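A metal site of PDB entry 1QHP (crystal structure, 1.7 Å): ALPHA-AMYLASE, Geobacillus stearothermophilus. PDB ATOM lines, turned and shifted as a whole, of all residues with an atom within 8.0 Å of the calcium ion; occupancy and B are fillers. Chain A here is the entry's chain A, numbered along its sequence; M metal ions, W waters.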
ATOM      1  N   PRO A 130       1.163   0.365 -11.079  1.00  0.00           N
ATOM      2  CA  PRO A 130       2.188   1.101 -10.363  1.00  0.00           C
ATOM      3  C   PRO A 130       2.262   0.888  -8.866  1.00  0.00           C
ATOM      4  O   PRO A 130       3.186   1.409  -8.236  1.00  0.00           O
ATOM      5  CB  PRO A 130       1.954   2.608 -10.674  1.00  0.00           C
ATOM      6  CG  PRO A 130       0.462   2.595 -10.907  1.00  0.00           C
ATOM      7  CD  PRO A 130       0.097   1.258 -11.535  1.00  0.00           C
ATOM      8  N   ASN A 131       1.320   0.152  -8.280  1.00  0.00           N
ATOM      9  CA  ASN A 131       1.345   0.023  -6.826  1.00  0.00           C
ATOM     10  C   ASN A 131       2.434  -0.882  -6.279  1.00  0.00           C
ATOM     11  O   ASN A 131       2.894  -0.677  -5.162  1.00  0.00           O
ATOM     12  CB  ASN A 131      -0.018  -0.510  -6.322  1.00  0.00           C
ATOM     13  CG  ASN A 131      -0.014  -0.573  -4.798  1.00  0.00           C
ATOM     14  OD1 ASN A 131       0.111   0.505  -4.214  1.00  0.00           O
ATOM     15  ND2 ASN A 131      -0.133  -1.735  -4.180  1.00  0.00           N
ATOM     16  N   HIS A 132       2.830  -1.902  -7.052  1.00  0.00           N
ATOM     17  CA  HIS A 132       3.744  -2.885  -6.442  1.00  0.00           C
ATOM     18  C   HIS A 132       4.535  -3.625  -7.491  1.00  0.00           C
ATOM     19  O   HIS A 132       4.198  -3.560  -8.668  1.00  0.00           O
ATOM     20  CB  HIS A 132       2.884  -3.868  -5.624  1.00  0.00           C
ATOM     21  CG  HIS A 132       1.684  -4.375  -6.367  1.00  0.00           C
ATOM     22  ND1 HIS A 132       0.427  -3.874  -6.084  1.00  0.00           N
ATOM     23  CD2 HIS A 132       1.535  -5.275  -7.347  1.00  0.00           C
ATOM     24  CE1 HIS A 132      -0.454  -4.448  -6.884  1.00  0.00           C
ATOM     25  NE2 HIS A 132       0.183  -5.294  -7.667  1.00  0.00           N
ATOM     26  N   HIS A 169       8.102   0.874   0.227  1.00  0.00           N
ATOM     27  CA  HIS A 169       7.639   1.181   1.574  1.00  0.00           C
ATOM     28  C   HIS A 169       7.927  -0.042   2.445  1.00  0.00           C
ATOM     29  O   HIS A 169       7.952  -1.170   1.950  1.00  0.00           O
ATOM     30  CB  HIS A 169       6.120   1.428   1.640  1.00  0.00           C
ATOM     31  CG  HIS A 169       5.706   2.639   0.853  1.00  0.00           C
ATOM     32  ND1 HIS A 169       4.565   2.599   0.060  1.00  0.00           N
ATOM     33  CD2 HIS A 169       6.239   3.869   0.708  1.00  0.00           C
ATOM     34  CE1 HIS A 169       4.420   3.782  -0.535  1.00  0.00           C
ATOM     35  NE2 HIS A 169       5.412   4.572  -0.159  1.00  0.00           N
ATOM     36  N   ILE A 174      -1.215  -4.454   5.060  1.00  0.00           N
ATOM     37  CA  ILE A 174      -2.500  -3.820   5.337  1.00  0.00           C
ATOM     38  C   ILE A 174      -3.291  -4.707   6.315  1.00  0.00           C
ATOM     39  O   ILE A 174      -3.342  -5.932   6.139  1.00  0.00           O
ATOM     40  CB  ILE A 174      -3.340  -3.650   4.056  1.00  0.00           C
ATOM     41  CG1 ILE A 174      -2.641  -2.632   3.123  1.00  0.00           C
ATOM     42  CG2 ILE A 174      -4.765  -3.220   4.369  1.00  0.00           C
ATOM     43  CD1 ILE A 174      -3.225  -2.617   1.718  1.00  0.00           C
ATOM     44  N   TYR A 181      -4.430   5.563   5.289  1.00  0.00           N
ATOM     45  CA  TYR A 181      -2.981   5.488   5.413  1.00  0.00           C
ATOM     46  C   TYR A 181      -2.550   4.040   5.170  1.00  0.00           C
ATOM     47  O   TYR A 181      -1.609   3.824   4.406  1.00  0.00           O
ATOM     48  CB  TYR A 181      -2.468   6.004   6.772  1.00  0.00           C
ATOM     49  CG  TYR A 181      -0.971   5.713   6.880  1.00  0.00           C
ATOM     50  CD1 TYR A 181      -0.046   6.483   6.207  1.00  0.00           C
ATOM     51  CD2 TYR A 181      -0.544   4.618   7.626  1.00  0.00           C
ATOM     52  CE1 TYR A 181       1.300   6.173   6.283  1.00  0.00           C
ATOM     53  CE2 TYR A 181       0.798   4.303   7.716  1.00  0.00           C
ATOM     54  CZ  TYR A 181       1.721   5.097   7.044  1.00  0.00           C
ATOM     55  OH  TYR A 181       3.055   4.774   7.103  1.00  0.00           O
ATOM     56  N   GLU A 182      -3.181   3.058   5.827  1.00  0.00           N
ATOM     57  CA  GLU A 182      -2.779   1.662   5.606  1.00  0.00           C
ATOM     58  C   GLU A 182      -2.946   1.239   4.155  1.00  0.00           C
ATOM     59  O   GLU A 182      -2.073   0.598   3.585  1.00  0.00           O
ATOM     60  CB  GLU A 182      -3.612   0.674   6.438  1.00  0.00           C
ATOM     61  CG  GLU A 182      -3.289   0.812   7.924  1.00  0.00           C
ATOM     62  CD  GLU A 182      -3.892  -0.337   8.718  1.00  0.00           C
ATOM     63  OE1 GLU A 182      -3.878  -1.485   8.251  1.00  0.00           O
ATOM     64  OE2 GLU A 182      -4.406  -0.080   9.826  1.00  0.00           O
ATOM     65  N   ALA A 183      -4.077   1.608   3.545  1.00  0.00           N
ATOM     66  CA  ALA A 183      -4.386   1.161   2.191  1.00  0.00           C
ATOM     67  C   ALA A 183      -3.311   1.616   1.202  1.00  0.00           C
ATOM     68  O   ALA A 183      -3.104   0.941   0.200  1.00  0.00           O
ATOM     69  CB  ALA A 183      -5.742   1.714   1.760  1.00  0.00           C
ATOM     70  N   GLN A 184      -2.693   2.762   1.464  1.00  0.00           N
ATOM     71  CA  GLN A 184      -1.691   3.301   0.568  1.00  0.00           C
ATOM     72  C   GLN A 184      -0.268   3.016   1.002  1.00  0.00           C
ATOM     73  O   GLN A 184       0.580   2.869   0.103  1.00  0.00           O
ATOM     74  CB  GLN A 184      -1.891   4.829   0.421  1.00  0.00           C
ATOM     75  CG  GLN A 184      -3.235   5.136  -0.251  1.00  0.00           C
ATOM     76  CD  GLN A 184      -3.583   6.611  -0.131  1.00  0.00           C
ATOM     77  OE1 GLN A 184      -3.432   7.388  -1.076  1.00  0.00           O
ATOM     78  NE2 GLN A 184      -4.061   7.015   1.053  1.00  0.00           N
ATOM     79  N   TRP A 185       0.092   3.029   2.269  1.00  0.00           N
ATOM     80  CA  TRP A 185       1.488   2.867   2.667  1.00  0.00           C
ATOM     81  C   TRP A 185       1.833   1.471   3.167  1.00  0.00           C
ATOM     82  O   TRP A 185       3.023   1.193   3.290  1.00  0.00           O
ATOM     83  CB  TRP A 185       1.858   3.952   3.717  1.00  0.00           C
ATOM     84  CG  TRP A 185       2.318   5.197   3.010  1.00  0.00           C
ATOM     85  CD1 TRP A 185       3.610   5.519   2.696  1.00  0.00           C
ATOM     86  CD2 TRP A 185       1.515   6.273   2.499  1.00  0.00           C
ATOM     87  NE1 TRP A 185       3.654   6.706   2.001  1.00  0.00           N
ATOM     88  CE2 TRP A 185       2.380   7.169   1.862  1.00  0.00           C
ATOM     89  CE3 TRP A 185       0.142   6.542   2.500  1.00  0.00           C
ATOM     90  CZ2 TRP A 185       1.929   8.351   1.243  1.00  0.00           C
ATOM     91  CZ3 TRP A 185      -0.310   7.694   1.891  1.00  0.00           C
ATOM     92  CH2 TRP A 185       0.587   8.590   1.256  1.00  0.00           C
ATOM     93  N   LYS A 186       0.847   0.618   3.400  1.00  0.00           N
ATOM     94  CA  LYS A 186       1.117  -0.749   3.833  1.00  0.00           C
ATOM     95  C   LYS A 186       0.906  -1.686   2.641  1.00  0.00           C
ATOM     96  O   LYS A 186       0.406  -1.275   1.596  1.00  0.00           O
ATOM     97  CB  LYS A 186       0.300  -1.179   5.059  1.00  0.00           C
ATOM     98  CG  LYS A 186       0.734  -0.333   6.273  1.00  0.00           C
ATOM     99  CD  LYS A 186       0.040  -0.820   7.537  1.00  0.00           C
ATOM    100  CE  LYS A 186       0.502   0.057   8.709  1.00  0.00           C
ATOM    101  NZ  LYS A 186       0.713  -0.780   9.926  1.00  0.00           N
ATOM    102  N   ASN A 187       1.357  -2.935   2.805  1.00  0.00           N
ATOM    103  CA  ASN A 187       1.373  -3.862   1.673  1.00  0.00           C
ATOM    104  C   ASN A 187       0.052  -4.535   1.325  1.00  0.00           C
ATOM    105  O   ASN A 187      -0.644  -5.036   2.188  1.00  0.00           O
ATOM    106  CB  ASN A 187       2.374  -5.005   1.951  1.00  0.00           C
ATOM    107  CG  ASN A 187       3.704  -4.530   2.488  1.00  0.00           C
ATOM    108  OD1 ASN A 187       4.216  -3.497   2.072  1.00  0.00           O
ATOM    109  ND2 ASN A 187       4.247  -5.308   3.433  1.00  0.00           N
ATOM    110  N   PHE A 188      -0.190  -4.631   0.018  1.00  0.00           N
ATOM    111  CA  PHE A 188      -1.325  -5.385  -0.516  1.00  0.00           C
ATOM    112  C   PHE A 188      -1.016  -6.851  -0.194  1.00  0.00           C
ATOM    113  O   PHE A 188       0.126  -7.261  -0.377  1.00  0.00           O
ATOM    114  CB  PHE A 188      -1.383  -5.201  -2.043  1.00  0.00           C
ATOM    115  CG  PHE A 188      -2.695  -5.521  -2.699  1.00  0.00           C
ATOM    116  CD1 PHE A 188      -3.091  -6.835  -2.901  1.00  0.00           C
ATOM    117  CD2 PHE A 188      -3.515  -4.494  -3.140  1.00  0.00           C
ATOM    118  CE1 PHE A 188      -4.303  -7.122  -3.511  1.00  0.00           C
ATOM    119  CE2 PHE A 188      -4.728  -4.778  -3.741  1.00  0.00           C
ATOM    120  CZ  PHE A 188      -5.115  -6.091  -3.932  1.00  0.00           C
ATOM    121  N   LEU A 196       2.609  -8.142  -1.480  1.00  0.00           N
ATOM    122  CA  LEU A 196       3.182  -7.584  -2.710  1.00  0.00           C
ATOM    123  C   LEU A 196       4.066  -6.405  -2.310  1.00  0.00           C
ATOM    124  O   LEU A 196       3.635  -5.547  -1.522  1.00  0.00           O
ATOM    125  CB  LEU A 196       2.077  -7.157  -3.681  1.00  0.00           C
ATOM    126  CG  LEU A 196       1.038  -8.238  -4.039  1.00  0.00           C
ATOM    127  CD1 LEU A 196       0.056  -7.669  -5.077  1.00  0.00           C
ATOM    128  CD2 LEU A 196       1.656  -9.510  -4.604  1.00  0.00           C
ATOM    129  N   ALA A 197       5.317  -6.385  -2.793  1.00  0.00           N
ATOM    130  CA  ALA A 197       6.248  -5.305  -2.429  1.00  0.00           C
ATOM    131  C   ALA A 197       5.732  -3.956  -2.899  1.00  0.00           C
ATOM    132  O   ALA A 197       5.556  -3.732  -4.085  1.00  0.00           O
ATOM    133  CB  ALA A 197       7.634  -5.597  -3.007  1.00  0.00           C
ATOM    134  N   ASP A 198       5.467  -3.091  -1.936  1.00  0.00           N
ATOM    135  CA  ASP A 198       4.806  -1.815  -2.194  1.00  0.00           C
ATOM    136  C   ASP A 198       5.779  -0.726  -2.641  1.00  0.00           C
ATOM    137  O   ASP A 198       6.668  -0.339  -1.879  1.00  0.00           O
ATOM    138  CB  ASP A 198       4.121  -1.416  -0.868  1.00  0.00           C
ATOM    139  CG  ASP A 198       2.966  -0.502  -1.134  1.00  0.00           C
ATOM    140  OD1 ASP A 198       2.045  -0.922  -1.896  1.00  0.00           O
ATOM    141  OD2 ASP A 198       2.930   0.646  -0.594  1.00  0.00           O
ATOM    142  N   LEU A 199       5.670  -0.344  -3.913  1.00  0.00           N
ATOM    143  CA  LEU A 199       6.577   0.658  -4.458  1.00  0.00           C
ATOM    144  C   LEU A 199       6.345   2.017  -3.790  1.00  0.00           C
ATOM    145  O   LEU A 199       5.217   2.374  -3.417  1.00  0.00           O
ATOM    146  CB  LEU A 199       6.365   0.770  -5.978  1.00  0.00           C
ATOM    147  CG  LEU A 199       6.844  -0.457  -6.768  1.00  0.00           C
ATOM    148  CD1 LEU A 199       6.340  -0.348  -8.203  1.00  0.00           C
ATOM    149  CD2 LEU A 199       8.364  -0.565  -6.756  1.00  0.00           C
ATOM    150  N   SER A 200       7.440   2.777  -3.644  1.00  0.00           N
ATOM    151  CA  SER A 200       7.342   4.113  -3.057  1.00  0.00           C
ATOM    152  C   SER A 200       7.244   5.098  -4.206  1.00  0.00           C
ATOM    153  O   SER A 200       8.268   5.477  -4.787  1.00  0.00           O
ATOM    154  CB  SER A 200       8.570   4.446  -2.197  1.00  0.00           C
ATOM    155  OG  SER A 200       8.393   5.758  -1.637  1.00  0.00           O
ATOM    156  N   GLN A 201       6.020   5.562  -4.515  1.00  0.00           N
ATOM    157  CA  GLN A 201       5.873   6.579  -5.561  1.00  0.00           C
ATOM    158  C   GLN A 201       6.366   7.938  -5.083  1.00  0.00           C
ATOM    159  O   GLN A 201       6.471   8.876  -5.876  1.00  0.00           O
ATOM    160  CB  GLN A 201       4.428   6.705  -6.054  1.00  0.00           C
ATOM    161  CG  GLN A 201       3.887   5.403  -6.650  1.00  0.00           C
ATOM    162  CD  GLN A 201       3.417   4.432  -5.585  1.00  0.00           C
ATOM    163  OE1 GLN A 201       3.242   4.782  -4.410  1.00  0.00           O
ATOM    164  NE2 GLN A 201       3.162   3.187  -5.986  1.00  0.00           N
ATOM    165  N   GLU A 202       6.731   8.063  -3.813  1.00  0.00           N
ATOM    166  CA  GLU A 202       7.286   9.274  -3.237  1.00  0.00           C
ATOM    167  C   GLU A 202       8.809   9.303  -3.414  1.00  0.00           C
ATOM    168  O   GLU A 202       9.448  10.308  -3.110  1.00  0.00           O
ATOM    169  CB  GLU A 202       6.912   9.437  -1.748  1.00  0.00           C
ATOM    170  CG  GLU A 202       5.397   9.412  -1.551  1.00  0.00           C
ATOM    171  CD  GLU A 202       4.823   7.999  -1.459  1.00  0.00           C
ATOM    172  OE1 GLU A 202       5.533   7.069  -1.058  1.00  0.00           O
ATOM    173  OE2 GLU A 202       3.651   7.826  -1.822  1.00  0.00           O
ATOM    174  N   ALA A 229      -5.356  -0.227  -9.027  1.00  0.00           N
ATOM    175  CA  ALA A 229      -5.309   0.073  -7.612  1.00  0.00           C
ATOM    176  C   ALA A 229      -4.981   1.505  -7.275  1.00  0.00           C
ATOM    177  O   ALA A 229      -4.118   1.763  -6.425  1.00  0.00           O
ATOM    178  CB  ALA A 229      -4.253  -0.891  -7.045  1.00  0.00           C
ATOM    179  N   LYS A 231      -6.563   3.486  -5.391  1.00  0.00           N
ATOM    180  CA  LYS A 231      -6.829   3.804  -3.986  1.00  0.00           C
ATOM    181  C   LYS A 231      -5.647   3.372  -3.106  1.00  0.00           C
ATOM    182  O   LYS A 231      -5.637   3.643  -1.915  1.00  0.00           O
ATOM    183  CB  LYS A 231      -8.122   3.142  -3.516  1.00  0.00           C
ATOM    184  CG  LYS A 231      -7.994   1.686  -3.111  1.00  0.00           C
ATOM    185  CD  LYS A 231      -9.340   1.017  -2.918  1.00  0.00           C
ATOM    186  CE  LYS A 231     -10.042   1.488  -1.662  1.00  0.00           C
ATOM    187  NZ  LYS A 231     -11.344   0.755  -1.476  1.00  0.00           N
ATOM    188  N   HIS A 232      -4.725   2.586  -3.684  1.00  0.00           N
ATOM    189  CA  HIS A 232      -3.611   2.044  -2.938  1.00  0.00           C
ATOM    190  C   HIS A 232      -2.342   2.833  -3.134  1.00  0.00           C
ATOM    191  O   HIS A 232      -1.361   2.434  -2.520  1.00  0.00           O
ATOM    192  CB  HIS A 232      -3.392   0.561  -3.327  1.00  0.00           C
ATOM    193  CG  HIS A 232      -4.537  -0.287  -2.837  1.00  0.00           C
ATOM    194  ND1 HIS A 232      -4.789  -0.434  -1.486  1.00  0.00           N
ATOM    195  CD2 HIS A 232      -5.500  -0.971  -3.495  1.00  0.00           C
ATOM    196  CE1 HIS A 232      -5.896  -1.182  -1.349  1.00  0.00           C
ATOM    197  NE2 HIS A 232      -6.350  -1.508  -2.550  1.00  0.00           N
ATOM    198  N   PHE A 233      -2.249   3.904  -3.912  1.00  0.00           N
ATOM    199  CA  PHE A 233      -1.008   4.697  -3.931  1.00  0.00           C
ATOM    200  C   PHE A 233      -1.458   6.157  -3.873  1.00  0.00           C
ATOM    201  O   PHE A 233      -2.602   6.442  -4.252  1.00  0.00           O
ATOM    202  CB  PHE A 233      -0.069   4.352  -5.073  1.00  0.00           C
ATOM    203  CG  PHE A 233      -0.660   4.586  -6.441  1.00  0.00           C
ATOM    204  CD1 PHE A 233      -1.366   3.590  -7.091  1.00  0.00           C
ATOM    205  CD2 PHE A 233      -0.486   5.813  -7.069  1.00  0.00           C
ATOM    206  CE1 PHE A 233      -1.919   3.808  -8.334  1.00  0.00           C
ATOM    207  CE2 PHE A 233      -1.026   6.033  -8.323  1.00  0.00           C
ATOM    208  CZ  PHE A 233      -1.745   5.034  -8.962  1.00  0.00           C
ATOM    209  N   ASN A 234      -0.607   7.080  -3.403  1.00  0.00           N
ATOM    210  CA  ASN A 234      -1.066   8.465  -3.244  1.00  0.00           C
ATOM    211  C   ASN A 234      -1.682   9.067  -4.491  1.00  0.00           C
ATOM    212  O   ASN A 234      -1.246   8.826  -5.608  1.00  0.00           O
ATOM    213  CB  ASN A 234       0.054   9.310  -2.627  1.00  0.00           C
ATOM    214  CG  ASN A 234       1.040   9.872  -3.638  1.00  0.00           C
ATOM    215  OD1 ASN A 234       0.647  10.796  -4.353  1.00  0.00           O
ATOM    216  ND2 ASN A 234       2.268   9.379  -3.671  1.00  0.00           N
HETATM  217 CA    CA M   1       0.904   1.450  -2.009  1.00  0.00          CA
HETATM  218  O   HOH W   1       1.823   3.777  -2.395  1.00  0.00           O
HETATM  219  O   HOH W   2      -0.641  -0.081  -0.618  1.00  0.00           O
HETATM  220  O   HOH W   3       2.782   1.453  -3.725  1.00  0.00           O
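O of His 232 is bound to the calcium ion, 2.5 Å away. The calcium ion is bound by OD1 of Asn 131, 2.5 Å away. Water W1 is bound to the calcium ion. The calcium ion is bound by water W3. The backbone carbonyl oxygen (O) of Gln 184 binds the calcium ion (2.6 Å). The calcium ion is bound by water W2 (2.6 Å). OD2 of Asp 198 is bound to the calcium ion (2.6 Å). The calcium ion is bound by OD1 of Asp 198 (2.6 Å).
Water W3 lies within hydrogen-bond range of the backbone carbonyl oxygen (O) of Asn 131 (2.6 Å), the backbone carbonyl oxygen (O) of Leu 199 (2.6 Å) and the side-chain amide nitrogen (NE2) of Gln 201 (2.9 Å).
Within 4 Å of the calcium ion: Asn 131, Gln 184, Asp 198 and His 232. Along chain A the residues within 4 Å of the calcium ion span positions 131 to 232.
ND1 of His 232 sits at hydrogen-bond distance from O of Ala 183, at 2.8 Å. The backbone NH of Leu 199 sits at hydrogen-bond distance from the backbone carbonyl oxygen of Asn 131 (3.1 Å). The side-chain amide nitrogen (ND2) of Asn 131 lies within hydrogen-bond range of a ring nitrogen (ND1) of His 132. OE1 of Gln 184 sits close to O of Phe 233, at 3.4 Å. N of His 169 lies within hydrogen-bond range of O of Asp 198, 2.8 Å away.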
